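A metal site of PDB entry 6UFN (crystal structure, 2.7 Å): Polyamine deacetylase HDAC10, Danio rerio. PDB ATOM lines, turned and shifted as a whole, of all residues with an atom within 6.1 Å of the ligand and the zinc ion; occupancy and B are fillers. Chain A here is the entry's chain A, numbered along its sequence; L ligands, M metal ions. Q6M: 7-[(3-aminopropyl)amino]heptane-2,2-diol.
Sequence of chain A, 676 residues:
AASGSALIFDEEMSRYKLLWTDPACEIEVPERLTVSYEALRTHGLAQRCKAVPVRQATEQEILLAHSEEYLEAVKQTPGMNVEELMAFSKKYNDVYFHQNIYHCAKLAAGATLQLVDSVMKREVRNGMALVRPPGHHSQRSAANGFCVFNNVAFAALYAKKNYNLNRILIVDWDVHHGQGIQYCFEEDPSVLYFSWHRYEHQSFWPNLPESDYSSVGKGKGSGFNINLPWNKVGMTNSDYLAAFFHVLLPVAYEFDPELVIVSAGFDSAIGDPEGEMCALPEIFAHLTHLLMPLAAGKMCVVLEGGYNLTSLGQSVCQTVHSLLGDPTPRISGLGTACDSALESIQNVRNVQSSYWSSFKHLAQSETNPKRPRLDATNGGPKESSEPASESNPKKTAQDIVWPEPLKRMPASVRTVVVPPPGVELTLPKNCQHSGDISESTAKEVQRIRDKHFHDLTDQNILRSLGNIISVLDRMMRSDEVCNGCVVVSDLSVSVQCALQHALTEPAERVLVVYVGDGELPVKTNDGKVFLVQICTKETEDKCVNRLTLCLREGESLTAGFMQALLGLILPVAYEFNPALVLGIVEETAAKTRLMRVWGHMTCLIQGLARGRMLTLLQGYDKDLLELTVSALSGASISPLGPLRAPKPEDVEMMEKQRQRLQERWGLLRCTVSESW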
ATOM      1  N   PRO A  23     -18.383  -9.941 -25.403  1.00  0.00           N
ATOM      2  CA  PRO A  23     -17.339  -8.907 -25.482  1.00  0.00           C
ATOM      3  C   PRO A  23     -17.061  -8.211 -24.153  1.00  0.00           C
ATOM      4  O   PRO A  23     -15.991  -7.615 -24.005  1.00  0.00           O
ATOM      5  CB  PRO A  23     -17.897  -7.919 -26.518  1.00  0.00           C
ATOM      6  CG  PRO A  23     -18.891  -8.718 -27.310  1.00  0.00           C
ATOM      7  CD  PRO A  23     -19.488  -9.693 -26.347  1.00  0.00           C
ATOM      8  N   ALA A  24     -17.981  -8.270 -23.189  1.00  0.00           N
ATOM      9  CA  ALA A  24     -17.765  -7.604 -21.912  1.00  0.00           C
ATOM     10  C   ALA A  24     -16.848  -8.401 -21.001  1.00  0.00           C
ATOM     11  O   ALA A  24     -16.201  -7.809 -20.119  1.00  0.00           O
ATOM     12  CB  ALA A  24     -19.104  -7.351 -21.218  1.00  0.00           C
ATOM     13  N   CYS A  25     -16.767  -9.718 -21.175  1.00  0.00           N
ATOM     14  CA  CYS A  25     -16.008 -10.583 -20.275  1.00  0.00           C
ATOM     15  C   CYS A  25     -14.810 -11.252 -20.943  1.00  0.00           C
ATOM     16  O   CYS A  25     -14.099 -12.004 -20.266  1.00  0.00           O
ATOM     17  CB  CYS A  25     -16.929 -11.656 -19.681  1.00  0.00           C
ATOM     18  SG  CYS A  25     -18.228 -11.023 -18.596  1.00  0.00           S
ATOM     19  N   ILE A  27     -11.948 -10.330 -21.567  1.00  0.00           N
ATOM     20  CA  ILE A  27     -10.627  -9.949 -21.083  1.00  0.00           C
ATOM     21  C   ILE A  27     -10.227 -10.680 -19.808  1.00  0.00           C
ATOM     22  O   ILE A  27      -9.046 -10.682 -19.449  1.00  0.00           O
ATOM     23  CB  ILE A  27     -10.545  -8.437 -20.851  1.00  0.00           C
ATOM     24  CG1 ILE A  27     -11.625  -7.999 -19.861  1.00  0.00           C
ATOM     25  CG2 ILE A  27     -10.673  -7.687 -22.172  1.00  0.00           C
ATOM     26  CD1 ILE A  27     -11.551  -6.551 -19.493  1.00  0.00           C
ATOM     27  N   ASP A  94     -22.186  -8.221 -16.110  1.00  0.00           N
ATOM     28  CA  ASP A  94     -20.818  -8.408 -16.603  1.00  0.00           C
ATOM     29  C   ASP A  94     -20.042  -9.434 -15.761  1.00  0.00           C
ATOM     30  O   ASP A  94     -19.013  -9.127 -15.155  1.00  0.00           O
ATOM     31  CB  ASP A  94     -20.073  -7.071 -16.669  1.00  0.00           C
ATOM     32  CG  ASP A  94     -20.501  -6.226 -17.854  1.00  0.00           C
ATOM     33  OD1 ASP A  94     -21.325  -6.714 -18.663  1.00  0.00           O
ATOM     34  OD2 ASP A  94     -20.006  -5.090 -17.986  1.00  0.00           O
ATOM     35  N   PRO A 134     -11.642 -12.167  -9.168  1.00  0.00           N
ATOM     36  CA  PRO A 134     -11.551 -11.012  -8.261  1.00  0.00           C
ATOM     37  C   PRO A 134     -12.761 -10.918  -7.346  1.00  0.00           C
ATOM     38  O   PRO A 134     -13.657 -11.766  -7.405  1.00  0.00           O
ATOM     39  CB  PRO A 134     -11.468  -9.815  -9.224  1.00  0.00           C
ATOM     40  CG  PRO A 134     -12.083 -10.311 -10.491  1.00  0.00           C
ATOM     41  CD  PRO A 134     -11.703 -11.760 -10.580  1.00  0.00           C
ATOM     42  N   GLY A 135     -12.825  -9.885  -6.511  1.00  0.00           N
ATOM     43  CA  GLY A 135     -13.879  -9.834  -5.523  1.00  0.00           C
ATOM     44  C   GLY A 135     -14.514  -8.493  -5.224  1.00  0.00           C
ATOM     45  O   GLY A 135     -15.661  -8.449  -4.756  1.00  0.00           O
ATOM     46  N   HIS A 136     -13.811  -7.387  -5.493  1.00  0.00           N
ATOM     47  CA  HIS A 136     -14.235  -6.106  -4.918  1.00  0.00           C
ATOM     48  C   HIS A 136     -15.547  -5.578  -5.517  1.00  0.00           C
ATOM     49  O   HIS A 136     -16.103  -4.628  -4.965  1.00  0.00           O
ATOM     50  CB  HIS A 136     -13.124  -5.068  -5.051  1.00  0.00           C
ATOM     51  CG  HIS A 136     -12.889  -4.570  -6.450  1.00  0.00           C
ATOM     52  ND1 HIS A 136     -12.229  -3.389  -6.713  1.00  0.00           N
ATOM     53  CD2 HIS A 136     -13.198  -5.101  -7.653  1.00  0.00           C
ATOM     54  CE1 HIS A 136     -12.153  -3.216  -8.021  1.00  0.00           C
ATOM     55  NE2 HIS A 136     -12.742  -4.240  -8.611  1.00  0.00           N
ATOM     56  N   HIS A 137     -16.047  -6.182  -6.590  1.00  0.00           N
ATOM     57  CA  HIS A 137     -17.370  -5.822  -7.097  1.00  0.00           C
ATOM     58  C   HIS A 137     -18.493  -6.670  -6.509  1.00  0.00           C
ATOM     59  O   HIS A 137     -19.655  -6.270  -6.569  1.00  0.00           O
ATOM     60  CB  HIS A 137     -17.421  -5.928  -8.625  1.00  0.00           C
ATOM     61  CG  HIS A 137     -16.526  -4.962  -9.333  1.00  0.00           C
ATOM     62  ND1 HIS A 137     -16.415  -3.639  -8.955  1.00  0.00           N
ATOM     63  CD2 HIS A 137     -15.716  -5.109 -10.403  1.00  0.00           C
ATOM     64  CE1 HIS A 137     -15.561  -3.020  -9.758  1.00  0.00           C
ATOM     65  NE2 HIS A 137     -15.124  -3.895 -10.651  1.00  0.00           N
ATOM     66  N   GLY A 145     -19.236  -7.865 -12.081  1.00  0.00           N
ATOM     67  CA  GLY A 145     -17.938  -7.518 -12.646  1.00  0.00           C
ATOM     68  C   GLY A 145     -16.847  -8.544 -12.422  1.00  0.00           C
ATOM     69  O   GLY A 145     -15.848  -8.242 -11.763  1.00  0.00           O
ATOM     70  N   PHE A 146     -17.033  -9.750 -12.957  1.00  0.00           N
ATOM     71  CA  PHE A 146     -16.112 -10.880 -12.863  1.00  0.00           C
ATOM     72  C   PHE A 146     -15.961 -11.422 -11.440  1.00  0.00           C
ATOM     73  O   PHE A 146     -15.220 -12.381 -11.245  1.00  0.00           O
ATOM     74  CB  PHE A 146     -14.708 -10.564 -13.393  1.00  0.00           C
ATOM     75  CG  PHE A 146     -14.688  -9.851 -14.719  1.00  0.00           C
ATOM     76  CD1 PHE A 146     -15.647 -10.117 -15.684  1.00  0.00           C
ATOM     77  CD2 PHE A 146     -13.707  -8.913 -14.995  1.00  0.00           C
ATOM     78  CE1 PHE A 146     -15.622  -9.453 -16.905  1.00  0.00           C
ATOM     79  CE2 PHE A 146     -13.679  -8.241 -16.204  1.00  0.00           C
ATOM     80  CZ  PHE A 146     -14.641  -8.513 -17.156  1.00  0.00           C
ATOM     81  N   CYS A 147     -16.630 -10.823 -10.459  1.00  0.00           N
ATOM     82  CA  CYS A 147     -16.458 -11.197  -9.062  1.00  0.00           C
ATOM     83  C   CYS A 147     -17.619 -12.067  -8.586  1.00  0.00           C
ATOM     84  O   CYS A 147     -18.785 -11.778  -8.883  1.00  0.00           O
ATOM     85  CB  CYS A 147     -16.341  -9.962  -8.177  1.00  0.00           C
ATOM     86  SG  CYS A 147     -15.096  -8.761  -8.720  1.00  0.00           S
ATOM     87  N   ASP A 174      -7.307  -0.584  -7.840  1.00  0.00           N
ATOM     88  CA  ASP A 174      -7.870  -1.049  -9.097  1.00  0.00           C
ATOM     89  C   ASP A 174      -8.542   0.102  -9.823  1.00  0.00           C
ATOM     90  O   ASP A 174      -9.015   1.058  -9.203  1.00  0.00           O
ATOM     91  CB  ASP A 174      -8.871  -2.182  -8.838  1.00  0.00           C
ATOM     92  CG  ASP A 174      -9.449  -2.766 -10.110  1.00  0.00           C
ATOM     93  OD1 ASP A 174      -8.967  -3.814 -10.564  1.00  0.00           O
ATOM     94  OD2 ASP A 174     -10.400  -2.167 -10.657  1.00  0.00           O
ATOM     95  N   VAL A 175      -8.573   0.026 -11.152  1.00  0.00           N
ATOM     96  CA  VAL A 175      -9.113   1.143 -11.933  1.00  0.00           C
ATOM     97  C   VAL A 175     -10.629   1.224 -11.873  1.00  0.00           C
ATOM     98  O   VAL A 175     -11.201   2.247 -12.245  1.00  0.00           O
ATOM     99  CB  VAL A 175      -8.665   1.076 -13.406  1.00  0.00           C
ATOM    100  CG1 VAL A 175      -9.474   0.029 -14.174  1.00  0.00           C
ATOM    101  CG2 VAL A 175      -8.773   2.449 -14.056  1.00  0.00           C
ATOM    102  N   HIS A 176     -11.298   0.164 -11.411  1.00  0.00           N
ATOM    103  CA  HIS A 176     -12.737   0.190 -11.207  1.00  0.00           C
ATOM    104  C   HIS A 176     -13.054   0.431  -9.732  1.00  0.00           C
ATOM    105  O   HIS A 176     -12.239   0.156  -8.850  1.00  0.00           O
ATOM    106  CB  HIS A 176     -13.377  -1.128 -11.659  1.00  0.00           C
ATOM    107  CG  HIS A 176     -13.102  -1.472 -13.094  1.00  0.00           C
ATOM    108  ND1 HIS A 176     -11.966  -2.131 -13.505  1.00  0.00           N
ATOM    109  CD2 HIS A 176     -13.840  -1.243 -14.213  1.00  0.00           C
ATOM    110  CE1 HIS A 176     -12.007  -2.295 -14.811  1.00  0.00           C
ATOM    111  NE2 HIS A 176     -13.122  -1.769 -15.270  1.00  0.00           N
ATOM    112  N   HIS A 177     -14.251   0.958  -9.478  1.00  0.00           N
ATOM    113  CA  HIS A 177     -14.682   1.235  -8.115  1.00  0.00           C
ATOM    114  C   HIS A 177     -15.192  -0.048  -7.476  1.00  0.00           C
ATOM    115  O   HIS A 177     -16.131  -0.677  -7.979  1.00  0.00           O
ATOM    116  CB  HIS A 177     -15.774   2.303  -8.101  1.00  0.00           C
ATOM    117  CG  HIS A 177     -16.325   2.581  -6.735  1.00  0.00           C
ATOM    118  ND1 HIS A 177     -17.676   2.595  -6.469  1.00  0.00           N
ATOM    119  CD2 HIS A 177     -15.701   2.840  -5.560  1.00  0.00           C
ATOM    120  CE1 HIS A 177     -17.866   2.863  -5.188  1.00  0.00           C
ATOM    121  NE2 HIS A 177     -16.686   3.012  -4.615  1.00  0.00           N
ATOM    122  N   TRP A 205     -18.215   2.355 -16.303  1.00  0.00           N
ATOM    123  CA  TRP A 205     -18.742   1.257 -15.494  1.00  0.00           C
ATOM    124  C   TRP A 205     -18.140   1.294 -14.089  1.00  0.00           C
ATOM    125  O   TRP A 205     -16.937   1.571 -13.936  1.00  0.00           O
ATOM    126  CB  TRP A 205     -18.427  -0.076 -16.179  1.00  0.00           C
ATOM    127  CG  TRP A 205     -19.131  -1.257 -15.589  1.00  0.00           C
ATOM    128  CD1 TRP A 205     -20.305  -1.810 -16.011  1.00  0.00           C
ATOM    129  CD2 TRP A 205     -18.691  -2.051 -14.473  1.00  0.00           C
ATOM    130  NE1 TRP A 205     -20.625  -2.889 -15.233  1.00  0.00           N
ATOM    131  CE2 TRP A 205     -19.648  -3.053 -14.274  1.00  0.00           C
ATOM    132  CE3 TRP A 205     -17.578  -1.998 -13.627  1.00  0.00           C
ATOM    133  CZ2 TRP A 205     -19.533  -4.010 -13.264  1.00  0.00           C
ATOM    134  CZ3 TRP A 205     -17.462  -2.941 -12.626  1.00  0.00           C
ATOM    135  CH2 TRP A 205     -18.437  -3.928 -12.448  1.00  0.00           C
ATOM    136  N   GLY A 265      -5.612  -4.132  -8.026  1.00  0.00           N
ATOM    137  CA  GLY A 265      -5.933  -4.275  -9.427  1.00  0.00           C
ATOM    138  C   GLY A 265      -4.961  -3.455 -10.251  1.00  0.00           C
ATOM    139  O   GLY A 265      -4.759  -2.263  -9.994  1.00  0.00           O
ATOM    140  N   ASP A 267      -5.175  -3.021 -13.590  1.00  0.00           N
ATOM    141  CA  ASP A 267      -5.768  -2.396 -14.766  1.00  0.00           C
ATOM    142  C   ASP A 267      -5.656  -0.891 -14.734  1.00  0.00           C
ATOM    143  O   ASP A 267      -6.068  -0.231 -15.704  1.00  0.00           O
ATOM    144  CB  ASP A 267      -7.236  -2.821 -14.903  1.00  0.00           C
ATOM    145  CG  ASP A 267      -7.979  -2.771 -13.584  1.00  0.00           C
ATOM    146  OD1 ASP A 267      -7.401  -2.294 -12.586  1.00  0.00           O
ATOM    147  OD2 ASP A 267      -9.146  -3.205 -13.552  1.00  0.00           O
ATOM    148  N   GLU A 274      -9.025  -1.560 -20.126  1.00  0.00           N
ATOM    149  CA  GLU A 274     -10.129  -1.063 -19.313  1.00  0.00           C
ATOM    150  C   GLU A 274      -9.834   0.316 -18.726  1.00  0.00           C
ATOM    151  O   GLU A 274     -10.668   1.219 -18.802  1.00  0.00           O
ATOM    152  CB  GLU A 274     -10.438  -2.048 -18.185  1.00  0.00           C
ATOM    153  CG  GLU A 274     -11.416  -3.141 -18.557  1.00  0.00           C
ATOM    154  CD  GLU A 274     -12.802  -2.625 -18.847  1.00  0.00           C
ATOM    155  OE1 GLU A 274     -13.151  -2.480 -20.037  1.00  0.00           O
ATOM    156  OE2 GLU A 274     -13.547  -2.344 -17.885  1.00  0.00           O
ATOM    157  N   GLU A 304      -6.713  -8.139  -7.940  1.00  0.00           N
ATOM    158  CA  GLU A 304      -8.042  -7.846  -8.445  1.00  0.00           C
ATOM    159  C   GLU A 304      -8.039  -7.875  -9.967  1.00  0.00           C
ATOM    160  O   GLU A 304      -8.124  -8.939 -10.582  1.00  0.00           O
ATOM    161  CB  GLU A 304      -8.532  -6.493  -7.934  1.00  0.00           C
ATOM    162  CG  GLU A 304      -8.717  -6.419  -6.421  1.00  0.00           C
ATOM    163  CD  GLU A 304     -10.045  -7.018  -5.963  1.00  0.00           C
ATOM    164  OE1 GLU A 304     -10.862  -7.396  -6.825  1.00  0.00           O
ATOM    165  OE2 GLU A 304     -10.269  -7.089  -4.732  1.00  0.00           O
ATOM    166  N   GLY A 305      -7.934  -6.700 -10.588  1.00  0.00           N
ATOM    167  CA  GLY A 305      -7.946  -6.576 -12.032  1.00  0.00           C
ATOM    168  C   GLY A 305      -6.551  -6.534 -12.626  1.00  0.00           C
ATOM    169  O   GLY A 305      -5.534  -6.787 -11.963  1.00  0.00           O
ATOM    170  N   GLY A 306      -6.503  -6.198 -13.918  1.00  0.00           N
ATOM    171  CA  GLY A 306      -5.265  -6.191 -14.673  1.00  0.00           C
ATOM    172  C   GLY A 306      -5.347  -7.101 -15.882  1.00  0.00           C
ATOM    173  O   GLY A 306      -5.359  -8.333 -15.727  1.00  0.00           O
ATOM    174  N   TYR A 307      -5.406  -6.521 -17.079  1.00  0.00           N
ATOM    175  CA  TYR A 307      -5.771  -7.282 -18.259  1.00  0.00           C
ATOM    176  C   TYR A 307      -4.791  -7.165 -19.428  1.00  0.00           C
ATOM    177  O   TYR A 307      -4.896  -7.949 -20.369  1.00  0.00           O
ATOM    178  CB  TYR A 307      -7.178  -6.880 -18.729  1.00  0.00           C
ATOM    179  CG  TYR A 307      -8.172  -6.963 -17.603  1.00  0.00           C
ATOM    180  CD1 TYR A 307      -8.783  -8.171 -17.294  1.00  0.00           C
ATOM    181  CD2 TYR A 307      -8.467  -5.858 -16.823  1.00  0.00           C
ATOM    182  CE1 TYR A 307      -9.678  -8.267 -16.245  1.00  0.00           C
ATOM    183  CE2 TYR A 307      -9.367  -5.935 -15.768  1.00  0.00           C
ATOM    184  CZ  TYR A 307      -9.970  -7.142 -15.487  1.00  0.00           C
ATOM    185  OH  TYR A 307     -10.866  -7.238 -14.438  1.00  0.00           O
HETATM  186  C11 Q6M L   1     -16.664  -3.971 -18.462  1.00  0.00           C
HETATM  187  C12 Q6M L   1     -16.951  -4.553 -19.870  1.00  0.00           C
HETATM  188  C13 Q6M L   1     -15.741  -4.360 -20.820  1.00  0.00           C
HETATM  189  C01 Q6M L   1     -11.626  -6.574 -10.637  1.00  0.00           C
HETATM  190  C02 Q6M L   1     -12.053  -5.598 -11.734  1.00  0.00           C
HETATM  191  C05 Q6M L   1     -13.261  -6.104 -12.545  1.00  0.00           C
HETATM  192  C06 Q6M L   1     -13.580  -5.308 -13.820  1.00  0.00           C
HETATM  193  C07 Q6M L   1     -15.071  -5.360 -14.212  1.00  0.00           C
HETATM  194  C08 Q6M L   1     -15.325  -5.073 -15.697  1.00  0.00           C
HETATM  195  C09 Q6M L   1     -16.727  -4.496 -16.012  1.00  0.00           C
HETATM  196  N10 Q6M L   1     -17.191  -4.852 -17.380  1.00  0.00           N
HETATM  197  N14 Q6M L   1     -16.176  -4.420 -22.228  1.00  0.00           N
HETATM  198  O03 Q6M L   1     -12.406  -4.359 -11.177  1.00  0.00           O
HETATM  199  O04 Q6M L   1     -11.005  -5.380 -12.625  1.00  0.00           O
HETATM  200 ZN    ZN M   1     -10.673  -3.416 -12.322  1.00  0.00          ZN
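The nearest printed residue that does not touch the zinc ion is Val 175 (4.1 Å).
The backbone carbonyl oxygen of Asp 94 is in hydrogen-bond range of the backbone NH of Phe 146, at 3.0 Å. The backbone NH (N) of His 136 sits at hydrogen-bond distance from the side-chain carboxylate (OE1) of Glu 304, 3.2 Å away. The side-chain carboxylate (OD1) of Asp 174 lies close to the backbone NH (N) of Gly 305 (3.1 Å). The backbone NH (N) of Gly 135 is in hydrogen-bond range of the side-chain carboxylate (OE1) of Glu 304 (3.2 Å). SG of Cys 147 is in hydrogen-bond range of O of Gly 145 (3.2 Å). The side-chain carboxylate (OD1) of Asp 267 is in hydrogen-bond range of the backbone NH (N) of Val 175. The side-chain carboxylate (OE2) of Glu 274 lies within hydrogen-bond range of a ring nitrogen (NE2) of His 176 (2.7 Å). The backbone NH (N) of His 137 is in hydrogen-bond range of the side-chain sulfur (SG) of Cys 147, at 3.5 Å.
Residues that only touch the ligand: Glu 274, Gly 305, Ala 24, Gly 145, Trp 205, Pro 134, Phe 146, Pro 23 and Glu 304. Hydrophobic or aromatic side chains within 4 Å of the ligand: Ala 24, Pro 134, His 136, His 137, Phe 146, His 176, Trp 205 and Tyr 307.
The zinc ion is bound by OD2 of Asp 267 (2.0 Å), O04 of the ligand (2.0 Å), OD2 of Asp 174 (2.1 Å), ND1 of His 176 (2.2 Å), O03 of the ligand (2.3 Å) and OD1 of Asp 174 (2.5 Å). The zinc ion has six donor atoms within binding distance.
OH of Tyr 307 lies close to O04 of the ligand, 2.6 Å away. A ring nitrogen (NE2) of His 137 lies close to an oxygen (O03) of the ligand, at 2.8 Å. The side-chain carboxylate of Asp 94 lies within salt-bridge range of a nitrogen (N10) of the ligand, 2.9 Å away. O03 of the ligand lies close to NE2 of His 136, 2.6 Å away.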
